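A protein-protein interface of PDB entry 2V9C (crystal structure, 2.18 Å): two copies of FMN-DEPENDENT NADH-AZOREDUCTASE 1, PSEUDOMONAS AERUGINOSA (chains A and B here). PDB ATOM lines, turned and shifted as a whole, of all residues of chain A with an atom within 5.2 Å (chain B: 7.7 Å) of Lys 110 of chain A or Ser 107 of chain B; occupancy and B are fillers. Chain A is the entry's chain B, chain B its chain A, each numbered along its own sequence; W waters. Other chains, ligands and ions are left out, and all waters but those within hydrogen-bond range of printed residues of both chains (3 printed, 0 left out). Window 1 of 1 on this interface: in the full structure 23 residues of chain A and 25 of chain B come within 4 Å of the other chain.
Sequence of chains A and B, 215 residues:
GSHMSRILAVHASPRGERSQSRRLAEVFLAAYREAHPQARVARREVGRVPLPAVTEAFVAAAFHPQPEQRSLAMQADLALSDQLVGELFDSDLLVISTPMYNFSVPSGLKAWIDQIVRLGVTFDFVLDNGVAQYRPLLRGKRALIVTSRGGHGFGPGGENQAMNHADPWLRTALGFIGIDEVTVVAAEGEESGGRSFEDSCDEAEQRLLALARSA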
ATOM      1  N   ALA A  53     -15.245  24.938 -14.459  1.00  0.00           N
ATOM      2  CA  ALA A  53     -14.186  24.252 -13.765  1.00  0.00           C
ATOM      3  C   ALA A  53     -14.804  23.361 -12.719  1.00  0.00           C
ATOM      4  O   ALA A  53     -15.919  23.561 -12.310  1.00  0.00           O
ATOM      5  CB  ALA A  53     -13.247  25.245 -13.108  1.00  0.00           C
ATOM      6  N   VAL A  54     -14.045  22.363 -12.314  1.00  0.00           N
ATOM      7  CA  VAL A  54     -14.435  21.460 -11.267  1.00  0.00           C
ATOM      8  C   VAL A  54     -14.547  22.273 -10.003  1.00  0.00           C
ATOM      9  O   VAL A  54     -13.690  23.051  -9.710  1.00  0.00           O
ATOM     10  CB  VAL A  54     -13.396  20.352 -11.115  1.00  0.00           C
ATOM     11  CG1 VAL A  54     -13.336  19.831  -9.728  1.00  0.00           C
ATOM     12  CG2 VAL A  54     -13.667  19.272 -12.064  1.00  0.00           C
ATOM     13  N   VAL A 105      -2.429  23.990 -22.881  1.00  0.00           N
ATOM     14  CA  VAL A 105      -3.649  24.172 -23.664  1.00  0.00           C
ATOM     15  C   VAL A 105      -4.533  25.259 -23.075  1.00  0.00           C
ATOM     16  O   VAL A 105      -4.389  25.595 -21.935  1.00  0.00           O
ATOM     17  CB  VAL A 105      -4.461  22.868 -23.767  1.00  0.00           C
ATOM     18  CG1 VAL A 105      -3.683  21.798 -24.424  1.00  0.00           C
ATOM     19  CG2 VAL A 105      -4.952  22.431 -22.439  1.00  0.00           C
ATOM     20  N   PRO A 106      -5.448  25.797 -23.856  1.00  0.00           N
ATOM     21  CA  PRO A 106      -6.342  26.807 -23.323  1.00  0.00           C
ATOM     22  C   PRO A 106      -7.117  26.231 -22.151  1.00  0.00           C
ATOM     23  O   PRO A 106      -7.334  25.040 -22.089  1.00  0.00           O
ATOM     24  CB  PRO A 106      -7.253  27.104 -24.498  1.00  0.00           C
ATOM     25  CG  PRO A 106      -6.530  26.719 -25.632  1.00  0.00           C
ATOM     26  CD  PRO A 106      -5.746  25.550 -25.265  1.00  0.00           C
ATOM     27  N   SER A 107      -7.507  27.082 -21.221  1.00  0.00           N
ATOM     28  CA  SER A 107      -8.141  26.638 -20.007  1.00  0.00           C
ATOM     29  C   SER A 107      -9.416  25.845 -20.147  1.00  0.00           C
ATOM     30  O   SER A 107      -9.724  25.045 -19.308  1.00  0.00           O
ATOM     31  CB  SER A 107      -8.259  27.756 -18.976  1.00  0.00           C
ATOM     32  OG  SER A 107      -9.103  28.776 -19.412  1.00  0.00           O
ATOM     33  N   GLY A 108     -10.136  26.051 -21.232  1.00  0.00           N
ATOM     34  CA  GLY A 108     -11.353  25.329 -21.481  1.00  0.00           C
ATOM     35  C   GLY A 108     -11.129  23.862 -21.752  1.00  0.00           C
ATOM     36  O   GLY A 108     -11.922  23.045 -21.370  1.00  0.00           O
ATOM     37  N   LEU A 109     -10.035  23.538 -22.418  1.00  0.00           N
ATOM     38  CA  LEU A 109      -9.693  22.166 -22.683  1.00  0.00           C
ATOM     39  C   LEU A 109      -9.282  21.447 -21.417  1.00  0.00           C
ATOM     40  O   LEU A 109      -9.603  20.305 -21.229  1.00  0.00           O
ATOM     41  CB  LEU A 109      -8.614  22.057 -23.747  1.00  0.00           C
ATOM     42  CG  LEU A 109      -8.199  20.661 -24.203  1.00  0.00           C
ATOM     43  CD1 LEU A 109      -9.377  19.774 -24.482  1.00  0.00           C
ATOM     44  CD2 LEU A 109      -7.301  20.724 -25.382  1.00  0.00           C
ATOM     45  N   LYS A 110      -8.559  22.129 -20.551  1.00  0.00           N
ATOM     46  CA  LYS A 110      -8.189  21.536 -19.304  1.00  0.00           C
ATOM     47  C   LYS A 110      -9.444  21.237 -18.494  1.00  0.00           C
ATOM     48  O   LYS A 110      -9.522  20.225 -17.842  1.00  0.00           O
ATOM     49  CB  LYS A 110      -7.239  22.439 -18.540  1.00  0.00           C
ATOM     50  CG  LYS A 110      -6.920  21.993 -17.142  1.00  0.00           C
ATOM     51  CD  LYS A 110      -5.856  20.937 -17.134  1.00  0.00           C
ATOM     52  CE  LYS A 110      -6.285  19.668 -16.470  1.00  0.00           C
ATOM     53  NZ  LYS A 110      -6.551  19.751 -15.049  1.00  0.00           N
ATOM     54  N   ALA A 111     -10.415  22.134 -18.555  1.00  0.00           N
ATOM     55  CA  ALA A 111     -11.678  21.953 -17.874  1.00  0.00           C
ATOM     56  C   ALA A 111     -12.509  20.797 -18.439  1.00  0.00           C
ATOM     57  O   ALA A 111     -13.209  20.139 -17.716  1.00  0.00           O
ATOM     58  CB  ALA A 111     -12.462  23.220 -17.858  1.00  0.00           C
ATOM     59  N   TRP A 112     -12.410  20.576 -19.735  1.00  0.00           N
ATOM     60  CA  TRP A 112     -13.095  19.478 -20.370  1.00  0.00           C
ATOM     61  C   TRP A 112     -12.556  18.171 -19.836  1.00  0.00           C
ATOM     62  O   TRP A 112     -13.301  17.329 -19.421  1.00  0.00           O
ATOM     63  CB  TRP A 112     -12.940  19.521 -21.879  1.00  0.00           C
ATOM     64  CG  TRP A 112     -13.638  18.414 -22.583  1.00  0.00           C
ATOM     65  CD1 TRP A 112     -14.949  18.328 -22.821  1.00  0.00           C
ATOM     66  CD2 TRP A 112     -13.055  17.239 -23.142  1.00  0.00           C
ATOM     67  NE1 TRP A 112     -15.237  17.192 -23.485  1.00  0.00           N
ATOM     68  CE2 TRP A 112     -14.086  16.499 -23.704  1.00  0.00           C
ATOM     69  CE3 TRP A 112     -11.762  16.747 -23.223  1.00  0.00           C
ATOM     70  CZ2 TRP A 112     -13.874  15.283 -24.332  1.00  0.00           C
ATOM     71  CZ3 TRP A 112     -11.551  15.548 -23.849  1.00  0.00           C
ATOM     72  CH2 TRP A 112     -12.596  14.831 -24.398  1.00  0.00           C
ATOM     73  N   ILE A 113     -11.246  18.029 -19.866  1.00  0.00           N
ATOM     74  CA  ILE A 113     -10.582  16.890 -19.299  1.00  0.00           C
ATOM     75  C   ILE A 113     -11.022  16.728 -17.857  1.00  0.00           C
ATOM     76  O   ILE A 113     -11.311  15.653 -17.433  1.00  0.00           O
ATOM     77  CB  ILE A 113      -9.047  17.040 -19.346  1.00  0.00           C
ATOM     78  CG1 ILE A 113      -8.538  17.070 -20.772  1.00  0.00           C
ATOM     79  CG2 ILE A 113      -8.371  15.964 -18.584  1.00  0.00           C
ATOM     80  CD1 ILE A 113      -8.446  15.754 -21.414  1.00  0.00           C
ATOM     81  N   ASP A 114     -11.090  17.812 -17.118  1.00  0.00           N
ATOM     82  CA  ASP A 114     -11.479  17.718 -15.738  1.00  0.00           C
ATOM     83  C   ASP A 114     -12.879  17.177 -15.512  1.00  0.00           C
ATOM     84  O   ASP A 114     -13.125  16.584 -14.497  1.00  0.00           O
ATOM     85  CB  ASP A 114     -11.207  19.010 -14.980  1.00  0.00           C
ATOM     86  CG  ASP A 114      -9.735  19.228 -14.696  1.00  0.00           C
ATOM     87  OD1 ASP A 114      -8.936  18.359 -15.001  1.00  0.00           O
ATOM     88  OD2 ASP A 114      -9.366  20.274 -14.171  1.00  0.00           O
ATOM     89  N   TRP A 169       0.794  16.238 -22.595  1.00  0.00           N
ATOM     90  CA  TRP A 169      -0.025  16.104 -21.414  1.00  0.00           C
ATOM     91  C   TRP A 169      -1.364  15.472 -21.779  1.00  0.00           C
ATOM     92  O   TRP A 169      -1.884  14.671 -21.048  1.00  0.00           O
ATOM     93  CB  TRP A 169      -0.243  17.419 -20.689  1.00  0.00           C
ATOM     94  CG  TRP A 169      -1.413  17.336 -19.825  1.00  0.00           C
ATOM     95  CD1 TRP A 169      -1.479  16.743 -18.628  1.00  0.00           C
ATOM     96  CD2 TRP A 169      -2.728  17.797 -20.115  1.00  0.00           C
ATOM     97  NE1 TRP A 169      -2.733  16.813 -18.131  1.00  0.00           N
ATOM     98  CE2 TRP A 169      -3.528  17.460 -19.027  1.00  0.00           C
ATOM     99  CE3 TRP A 169      -3.305  18.471 -21.187  1.00  0.00           C
ATOM    100  CZ2 TRP A 169      -4.867  17.776 -18.970  1.00  0.00           C
ATOM    101  CZ3 TRP A 169      -4.629  18.774 -21.126  1.00  0.00           C
ATOM    102  CH2 TRP A 169      -5.396  18.428 -20.034  1.00  0.00           C
ATOM    103  N   ALA B  12      -5.287  27.918  -5.905  1.00  0.00           N
ATOM    104  CA  ALA B  12      -5.945  27.257  -7.010  1.00  0.00           C
ATOM    105  C   ALA B  12      -6.879  26.097  -6.717  1.00  0.00           C
ATOM    106  O   ALA B  12      -7.552  25.613  -7.599  1.00  0.00           O
ATOM    107  CB  ALA B  12      -4.964  26.884  -8.055  1.00  0.00           C
ATOM    108  N   PRO B  14     -10.214  24.344  -5.505  1.00  0.00           N
ATOM    109  CA  PRO B  14     -11.614  24.698  -5.355  1.00  0.00           C
ATOM    110  C   PRO B  14     -12.120  24.356  -3.973  1.00  0.00           C
ATOM    111  O   PRO B  14     -13.183  24.769  -3.605  1.00  0.00           O
ATOM    112  CB  PRO B  14     -12.298  23.819  -6.395  1.00  0.00           C
ATOM    113  CG  PRO B  14     -11.334  22.833  -6.763  1.00  0.00           C
ATOM    114  CD  PRO B  14     -10.031  23.445  -6.641  1.00  0.00           C
ATOM    115  N   VAL B  46      -8.279  31.708  -7.407  1.00  0.00           N
ATOM    116  CA  VAL B  46      -8.495  31.206  -8.756  1.00  0.00           C
ATOM    117  C   VAL B  46      -9.083  29.808  -8.770  1.00  0.00           C
ATOM    118  O   VAL B  46      -9.241  29.209  -9.807  1.00  0.00           O
ATOM    119  CB  VAL B  46      -7.227  31.237  -9.626  1.00  0.00           C
ATOM    120  CG1 VAL B  46      -6.622  32.593  -9.669  1.00  0.00           C
ATOM    121  CG2 VAL B  46      -6.249  30.195  -9.213  1.00  0.00           C
ATOM    122  N   GLY B  47      -9.402  29.298  -7.598  1.00  0.00           N
ATOM    123  CA  GLY B  47      -9.948  27.971  -7.475  1.00  0.00           C
ATOM    124  C   GLY B  47     -11.400  27.926  -7.084  1.00  0.00           C
ATOM    125  O   GLY B  47     -12.156  27.172  -7.638  1.00  0.00           O
ATOM    126  N   LEU B  51     -12.436  32.060 -13.114  1.00  0.00           N
ATOM    127  CA  LEU B  51     -11.572  33.028 -13.730  1.00  0.00           C
ATOM    128  C   LEU B  51     -11.709  32.866 -15.219  1.00  0.00           C
ATOM    129  O   LEU B  51     -11.465  31.812 -15.740  1.00  0.00           O
ATOM    130  CB  LEU B  51     -10.139  32.754 -13.320  1.00  0.00           C
ATOM    131  CG  LEU B  51      -9.242  33.968 -13.237  1.00  0.00           C
ATOM    132  CD1 LEU B  51      -9.594  34.757 -12.048  1.00  0.00           C
ATOM    133  CD2 LEU B  51      -7.822  33.579 -13.195  1.00  0.00           C
ATOM    134  N   PRO B  52     -12.122  33.930 -15.877  1.00  0.00           N
ATOM    135  CA  PRO B  52     -12.329  33.928 -17.308  1.00  0.00           C
ATOM    136  C   PRO B  52     -11.176  33.382 -18.105  1.00  0.00           C
ATOM    137  O   PRO B  52     -10.016  33.656 -17.849  1.00  0.00           O
ATOM    138  CB  PRO B  52     -12.530  35.397 -17.630  1.00  0.00           C
ATOM    139  CG  PRO B  52     -12.588  36.098 -16.350  1.00  0.00           C
ATOM    140  CD  PRO B  52     -12.698  35.125 -15.273  1.00  0.00           C
ATOM    141  N   ALA B  53     -11.541  32.591 -19.091  1.00  0.00           N
ATOM    142  CA  ALA B  53     -10.624  32.029 -20.027  1.00  0.00           C
ATOM    143  C   ALA B  53     -10.360  33.075 -21.067  1.00  0.00           C
ATOM    144  O   ALA B  53     -11.118  33.989 -21.238  1.00  0.00           O
ATOM    145  CB  ALA B  53     -11.229  30.822 -20.670  1.00  0.00           C
ATOM    146  N   THR B  98      -1.683  24.717  -5.226  1.00  0.00           N
ATOM    147  CA  THR B  98      -2.440  23.994  -6.231  1.00  0.00           C
ATOM    148  C   THR B  98      -2.380  22.492  -6.023  1.00  0.00           C
ATOM    149  O   THR B  98      -1.366  21.948  -5.597  1.00  0.00           O
ATOM    150  CB  THR B  98      -1.944  24.322  -7.657  1.00  0.00           C
ATOM    151  OG1 THR B  98      -2.748  23.631  -8.618  1.00  0.00           O
ATOM    152  CG2 THR B  98      -0.494  23.906  -7.832  1.00  0.00           C
ATOM    153  N   PRO B  99      -3.482  21.826  -6.334  1.00  0.00           N
ATOM    154  CA  PRO B  99      -3.511  20.366  -6.342  1.00  0.00           C
ATOM    155  C   PRO B  99      -3.194  19.895  -7.751  1.00  0.00           C
ATOM    156  O   PRO B  99      -3.277  20.687  -8.685  1.00  0.00           O
ATOM    157  CB  PRO B  99      -4.968  20.050  -6.002  1.00  0.00           C
ATOM    158  CG  PRO B  99      -5.726  21.229  -6.484  1.00  0.00           C
ATOM    159  CD  PRO B  99      -4.832  22.408  -6.264  1.00  0.00           C
ATOM    160  N   MET B 100      -2.830  18.629  -7.902  1.00  0.00           N
ATOM    161  CA  MET B 100      -2.628  18.067  -9.226  1.00  0.00           C
ATOM    162  C   MET B 100      -3.953  17.497  -9.709  1.00  0.00           C
ATOM    163  O   MET B 100      -4.468  16.544  -9.134  1.00  0.00           O
ATOM    164  CB  MET B 100      -1.573  16.967  -9.194  1.00  0.00           C
ATOM    165  CG  MET B 100      -1.600  16.076 -10.418  1.00  0.00           C
ATOM    166  SD  MET B 100      -0.227  14.922 -10.484  1.00  0.00           S
ATOM    167  CE  MET B 100       1.077  15.974 -11.104  1.00  0.00           C
ATOM    168  N   TYR B 101      -4.511  18.086 -10.759  1.00  0.00           N
ATOM    169  CA  TYR B 101      -5.778  17.611 -11.287  1.00  0.00           C
ATOM    170  C   TYR B 101      -5.502  17.016 -12.652  1.00  0.00           C
ATOM    171  O   TYR B 101      -5.124  17.725 -13.553  1.00  0.00           O
ATOM    172  CB  TYR B 101      -6.767  18.772 -11.447  1.00  0.00           C
ATOM    173  CG  TYR B 101      -7.633  19.072 -10.245  1.00  0.00           C
ATOM    174  CD1 TYR B 101      -7.402  18.469  -9.031  1.00  0.00           C
ATOM    175  CD2 TYR B 101      -8.678  19.970 -10.332  1.00  0.00           C
ATOM    176  CE1 TYR B 101      -8.185  18.742  -7.949  1.00  0.00           C
ATOM    177  CE2 TYR B 101      -9.460  20.247  -9.252  1.00  0.00           C
ATOM    178  CZ  TYR B 101      -9.212  19.631  -8.062  1.00  0.00           C
ATOM    179  OH  TYR B 101      -9.988  19.894  -6.980  1.00  0.00           O
ATOM    180  N   ASN B 102      -5.685  15.713 -12.799  1.00  0.00           N
ATOM    181  CA  ASN B 102      -5.459  15.055 -14.078  1.00  0.00           C
ATOM    182  C   ASN B 102      -4.126  15.374 -14.737  1.00  0.00           C
ATOM    183  O   ASN B 102      -4.042  15.737 -15.901  1.00  0.00           O
ATOM    184  CB  ASN B 102      -6.644  15.247 -15.013  1.00  0.00           C
ATOM    185  CG  ASN B 102      -7.913  14.664 -14.445  1.00  0.00           C
ATOM    186  OD1 ASN B 102      -7.966  13.493 -14.116  1.00  0.00           O
ATOM    187  ND2 ASN B 102      -8.927  15.486 -14.300  1.00  0.00           N
ATOM    188  N   PHE B 103      -3.084  15.207 -13.944  1.00  0.00           N
ATOM    189  CA  PHE B 103      -1.709  15.373 -14.352  1.00  0.00           C
ATOM    190  C   PHE B 103      -1.284  16.809 -14.679  1.00  0.00           C
ATOM    191  O   PHE B 103      -0.250  17.031 -15.258  1.00  0.00           O
ATOM    192  CB  PHE B 103      -1.331  14.355 -15.431  1.00  0.00           C
ATOM    193  CG  PHE B 103      -1.793  12.949 -15.125  1.00  0.00           C
ATOM    194  CD1 PHE B 103      -1.120  12.162 -14.219  1.00  0.00           C
ATOM    195  CD2 PHE B 103      -2.907  12.421 -15.731  1.00  0.00           C
ATOM    196  CE1 PHE B 103      -1.554  10.902 -13.929  1.00  0.00           C
ATOM    197  CE2 PHE B 103      -3.334  11.167 -15.434  1.00  0.00           C
ATOM    198  CZ  PHE B 103      -2.659  10.412 -14.535  1.00  0.00           C
ATOM    199  N   SER B 104      -2.087  17.771 -14.261  1.00  0.00           N
ATOM    200  CA  SER B 104      -1.815  19.162 -14.509  1.00  0.00           C
ATOM    201  C   SER B 104      -2.419  19.956 -13.386  1.00  0.00           C
ATOM    202  O   SER B 104      -2.582  19.453 -12.313  1.00  0.00           O
ATOM    203  CB  SER B 104      -2.416  19.580 -15.840  1.00  0.00           C
ATOM    204  OG  SER B 104      -2.134  20.922 -16.115  1.00  0.00           O
ATOM    205  N   VAL B 105      -2.752  21.204 -13.631  1.00  0.00           N
ATOM    206  CA  VAL B 105      -3.351  22.044 -12.612  1.00  0.00           C
ATOM    207  C   VAL B 105      -4.836  22.245 -12.900  1.00  0.00           C
ATOM    208  O   VAL B 105      -5.258  22.094 -14.007  1.00  0.00           O
ATOM    209  CB  VAL B 105      -2.641  23.421 -12.521  1.00  0.00           C
ATOM    210  CG1 VAL B 105      -1.166  23.265 -12.279  1.00  0.00           C
ATOM    211  CG2 VAL B 105      -2.879  24.242 -13.738  1.00  0.00           C
ATOM    212  N   PRO B 106      -5.615  22.606 -11.901  1.00  0.00           N
ATOM    213  CA  PRO B 106      -7.007  22.956 -12.127  1.00  0.00           C
ATOM    214  C   PRO B 106      -7.114  24.020 -13.218  1.00  0.00           C
ATOM    215  O   PRO B 106      -6.212  24.813 -13.359  1.00  0.00           O
ATOM    216  CB  PRO B 106      -7.418  23.533 -10.787  1.00  0.00           C
ATOM    217  CG  PRO B 106      -6.582  22.874  -9.845  1.00  0.00           C
ATOM    218  CD  PRO B 106      -5.283  22.657 -10.478  1.00  0.00           C
ATOM    219  N   SER B 107      -8.199  24.026 -13.970  1.00  0.00           N
ATOM    220  CA  SER B 107      -8.357  24.959 -15.073  1.00  0.00           C
ATOM    221  C   SER B 107      -8.305  26.442 -14.738  1.00  0.00           C
ATOM    222  O   SER B 107      -7.872  27.228 -15.545  1.00  0.00           O
ATOM    223  CB  SER B 107      -9.570  24.616 -15.945  1.00  0.00           C
ATOM    224  OG  SER B 107     -10.763  24.728 -15.233  1.00  0.00           O
ATOM    225  N   GLY B 108      -8.720  26.794 -13.532  1.00  0.00           N
ATOM    226  CA  GLY B 108      -8.648  28.148 -13.056  1.00  0.00           C
ATOM    227  C   GLY B 108      -7.243  28.712 -12.997  1.00  0.00           C
ATOM    228  O   GLY B 108      -7.041  29.851 -13.305  1.00  0.00           O
ATOM    229  N   LEU B 109      -6.279  27.901 -12.594  1.00  0.00           N
ATOM    230  CA  LEU B 109      -4.893  28.318 -12.532  1.00  0.00           C
ATOM    231  C   LEU B 109      -4.309  28.490 -13.911  1.00  0.00           C
ATOM    232  O   LEU B 109      -3.497  29.353 -14.137  1.00  0.00           O
ATOM    233  CB  LEU B 109      -4.057  27.358 -11.701  1.00  0.00           C
ATOM    234  CG  LEU B 109      -2.588  27.709 -11.486  1.00  0.00           C
ATOM    235  CD1 LEU B 109      -2.419  29.084 -10.899  1.00  0.00           C
ATOM    236  CD2 LEU B 109      -1.894  26.691 -10.662  1.00  0.00           C
ATOM    237  N   LYS B 110      -4.740  27.654 -14.834  1.00  0.00           N
ATOM    238  CA  LYS B 110      -4.325  27.758 -16.208  1.00  0.00           C
ATOM    239  C   LYS B 110      -4.840  29.068 -16.782  1.00  0.00           C
ATOM    240  O   LYS B 110      -4.168  29.719 -17.544  1.00  0.00           O
ATOM    241  CB  LYS B 110      -4.854  26.580 -17.010  1.00  0.00           C
ATOM    242  CG  LYS B 110      -4.593  26.668 -18.483  1.00  0.00           C
ATOM    243  CD  LYS B 110      -3.194  26.258 -18.824  1.00  0.00           C
ATOM    244  CE  LYS B 110      -2.410  27.346 -19.496  1.00  0.00           C
ATOM    245  NZ  LYS B 110      -2.557  27.397 -20.939  1.00  0.00           N
ATOM    246  N   ALA B 111      -6.043  29.445 -16.392  1.00  0.00           N
ATOM    247  CA  ALA B 111      -6.637  30.664 -16.863  1.00  0.00           C
ATOM    248  C   ALA B 111      -5.913  31.861 -16.279  1.00  0.00           C
ATOM    249  O   ALA B 111      -5.788  32.871 -16.920  1.00  0.00           O
ATOM    250  CB  ALA B 111      -8.087  30.701 -16.542  1.00  0.00           C
ATOM    251  N   TRP B 112      -5.418  31.735 -15.059  1.00  0.00           N
ATOM    252  CA  TRP B 112      -4.685  32.814 -14.433  1.00  0.00           C
ATOM    253  C   TRP B 112      -3.394  33.070 -15.181  1.00  0.00           C
ATOM    254  O   TRP B 112      -3.049  34.194 -15.455  1.00  0.00           O
ATOM    255  CB  TRP B 112      -4.419  32.526 -12.967  1.00  0.00           C
ATOM    256  CG  TRP B 112      -3.663  33.616 -12.270  1.00  0.00           C
ATOM    257  CD1 TRP B 112      -4.155  34.788 -11.841  1.00  0.00           C
ATOM    258  CD2 TRP B 112      -2.281  33.622 -11.937  1.00  0.00           C
ATOM    259  NE1 TRP B 112      -3.185  35.523 -11.264  1.00  0.00           N
ATOM    260  CE2 TRP B 112      -2.016  34.831 -11.311  1.00  0.00           C
ATOM    261  CE3 TRP B 112      -1.242  32.721 -12.116  1.00  0.00           C
ATOM    262  CZ2 TRP B 112      -0.760  35.166 -10.850  1.00  0.00           C
ATOM    263  CZ3 TRP B 112      -0.001  33.054 -11.659  1.00  0.00           C
ATOM    264  CH2 TRP B 112       0.233  34.263 -11.037  1.00  0.00           C
ATOM    265  N   ILE B 113      -2.697  32.002 -15.517  1.00  0.00           N
ATOM    266  CA  ILE B 113      -1.497  32.107 -16.301  1.00  0.00           C
ATOM    267  C   ILE B 113      -1.793  32.797 -17.621  1.00  0.00           C
ATOM    268  O   ILE B 113      -1.086  33.696 -18.021  1.00  0.00           O
ATOM    269  CB  ILE B 113      -0.867  30.732 -16.541  1.00  0.00           C
ATOM    270  CG1 ILE B 113      -0.222  30.199 -15.268  1.00  0.00           C
ATOM    271  CG2 ILE B 113       0.094  30.758 -17.677  1.00  0.00           C
ATOM    272  CD1 ILE B 113       0.861  31.038 -14.705  1.00  0.00           C
ATOM    273  N   ASP B 114      -2.850  32.361 -18.286  1.00  0.00           N
ATOM    274  CA  ASP B 114      -3.228  32.884 -19.587  1.00  0.00           C
ATOM    275  C   ASP B 114      -3.536  34.365 -19.535  1.00  0.00           C
ATOM    276  O   ASP B 114      -3.403  35.047 -20.517  1.00  0.00           O
ATOM    277  CB  ASP B 114      -4.381  32.087 -20.211  1.00  0.00           C
ATOM    278  CG  ASP B 114      -3.954  30.721 -20.719  1.00  0.00           C
ATOM    279  OD1 ASP B 114      -2.767  30.492 -20.872  1.00  0.00           O
ATOM    280  OD2 ASP B 114      -4.803  29.870 -20.974  1.00  0.00           O
ATOM    281  N   HIS B 165       2.676  17.220 -15.328  1.00  0.00           N
ATOM    282  CA  HIS B 165       2.557  18.391 -16.163  1.00  0.00           C
ATOM    283  C   HIS B 165       1.934  19.505 -15.380  1.00  0.00           C
ATOM    284  O   HIS B 165       1.380  20.412 -15.932  1.00  0.00           O
ATOM    285  CB  HIS B 165       1.754  18.083 -17.411  1.00  0.00           C
ATOM    286  CG  HIS B 165       2.383  17.042 -18.267  1.00  0.00           C
ATOM    287  ND1 HIS B 165       3.423  17.313 -19.117  1.00  0.00           N
ATOM    288  CD2 HIS B 165       2.150  15.720 -18.370  1.00  0.00           C
ATOM    289  CE1 HIS B 165       3.796  16.206 -19.719  1.00  0.00           C
ATOM    290  NE2 HIS B 165       3.037  15.225 -19.284  1.00  0.00           N
HETATM  291  O   HOH W   1      -7.415  30.096 -21.085  1.00  0.00           O
HETATM  292  O   HOH W   2     -11.757  14.732 -13.100  1.00  0.00           O
HETATM  293  O   HOH W   3     -10.957  22.435 -13.619  1.00  0.00           O
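Of chain B, only Tyr 101, Ser 104, Val 105 and Ser 107 come within 4 Å of Lys 110 of chain A.
Of the printed residues of chain A, Pro 14 of chain B touches Val 54 (3.7 Å).
Printed residues of chain B within 4 Å of Val 105 of chain A: Lys 110 (2.8 Å).
Of the printed residues of chain A, Ser 104 of chain B touches Lys 110 (3.9 Å) and Trp 169 (3.6 Å).
NZ of Lys 110 of chain A lies within salt-bridge range of OD1 of Asp 114 of chain A, at 2.8 Å.
The side-chain carboxylate (OD1) of Asp 114 of chain B is in salt-bridge range of the side-chain amino group (NZ) of Lys 110 of chain B (3.1 Å).
The backbone NH (N) of His 165 of chain B sits at hydrogen-bond distance from the backbone carbonyl oxygen (O) of Phe 103 of chain B (2.9 Å).
Hydrophobic or aromatic side chains of chain A within 4 Å of the printed part of chain B: Ala 53, Val 54, Ala 111 and Trp 169.
Of the 25 printed residues of chain B, 12 touch a printed residue of chain A.
Along chain B the printed residues that touch a printed residue of chain A span positions 14 to 165.
Among the printed residues, 22 pairs touch across the chains.
Among the printed residues, no Asp or Glu carboxylate lies within 4 Å of a Lys or Arg side-chain nitrogen of the other chain.
Ala 53 of chain A touches Ser 107 of chain B, and with the chains exchanged Ser 107 of chain A touches Ala 53 of chain B.
Ser 107 of chain A touches its own counterpart, Ser 107 of chain B.
Ser 107 of chain A touches Lys 110 of chain B, and with the chains exchanged Lys 110 of chain A touches Ser 107 of chain B.
Ser 107 of chain A touches Asp 114 of chain B, and with the chains exchanged Asp 114 of chain A touches Ser 107 of chain B.
Of the 22 pairs that touch across the chains among the printed residues, 11 have their exchanged pair printed and touching as well.
The side-chain amide nitrogen (ND2) of Asn 102 of chain B is in hydrogen-bond range of the side-chain carboxylate (OD1) of Asp 114 of chain A.
The side-chain amino group (NZ) of Lys 110 of chain B sits at hydrogen-bond distance from the backbone carbonyl oxygen (O) of Val 105 of chain A, 2.8 Å away.
O of Tyr 101 of chain B lies within hydrogen-bond range of NZ of Lys 110 of chain A (2.9 Å).
The backbone carbonyl oxygen (O) of Val 105 of chain B sits at hydrogen-bond distance from the side-chain amino group (NZ) of Lys 110 of chain A.
O of Asn 102 of chain B is in hydrogen-bond range of NE1 of Trp 169 of chain A.
Water W1 lies within hydrogen-bond range of OD2 of Asp 114 of chain B (2.6 Å) and OG of Ser 107 of chain A (2.7 Å).
Water W2 lies within hydrogen-bond range of O of Asp 114 of chain A (2.7 Å) and ND2 of Asn 102 of chain B (3.2 Å).
Water W3 lies within hydrogen-bond range of the side-chain carboxylate (OD2) of Asp 114 of chain A (2.7 Å), the side-chain hydroxyl (OG) of Ser 107 of chain B (2.8 Å) and the backbone NH (N) of Val 54 of chain A (3.4 Å).
Among the printed residues, merely in contact across the chains: Ala 53 of chain A with Ser 107 of chain B, Val 54 of chain A with Pro 14 of chain B, Val 54 of chain A with Tyr 101 of chain B, Ser 107 of chain A with Ala 53 of chain B, Ser 107 of chain A with Ser 107 of chain B, Ser 107 of chain A with Lys 110 of chain B, Ser 107 of chain A with Ala 111 of chain B, Ser 107 of chain A with Asp 114 of chain B, Lys 110 of chain A with Ser 104 of chain B, Lys 110 of chain A with Ser 107 of chain B, Ala 111 of chain A with Ser 107 of chain B, Ile 113 of chain A with Asn 102 of chain B, Asp 114 of chain A with Tyr 101 of chain B, Asp 114 of chain A with Ser 107 of chain B, Trp 169 of chain A with Phe 103 of chain B, Trp 169 of chain A with Ser 104 of chain B and Trp 169 of chain A with His 165 of chain B.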
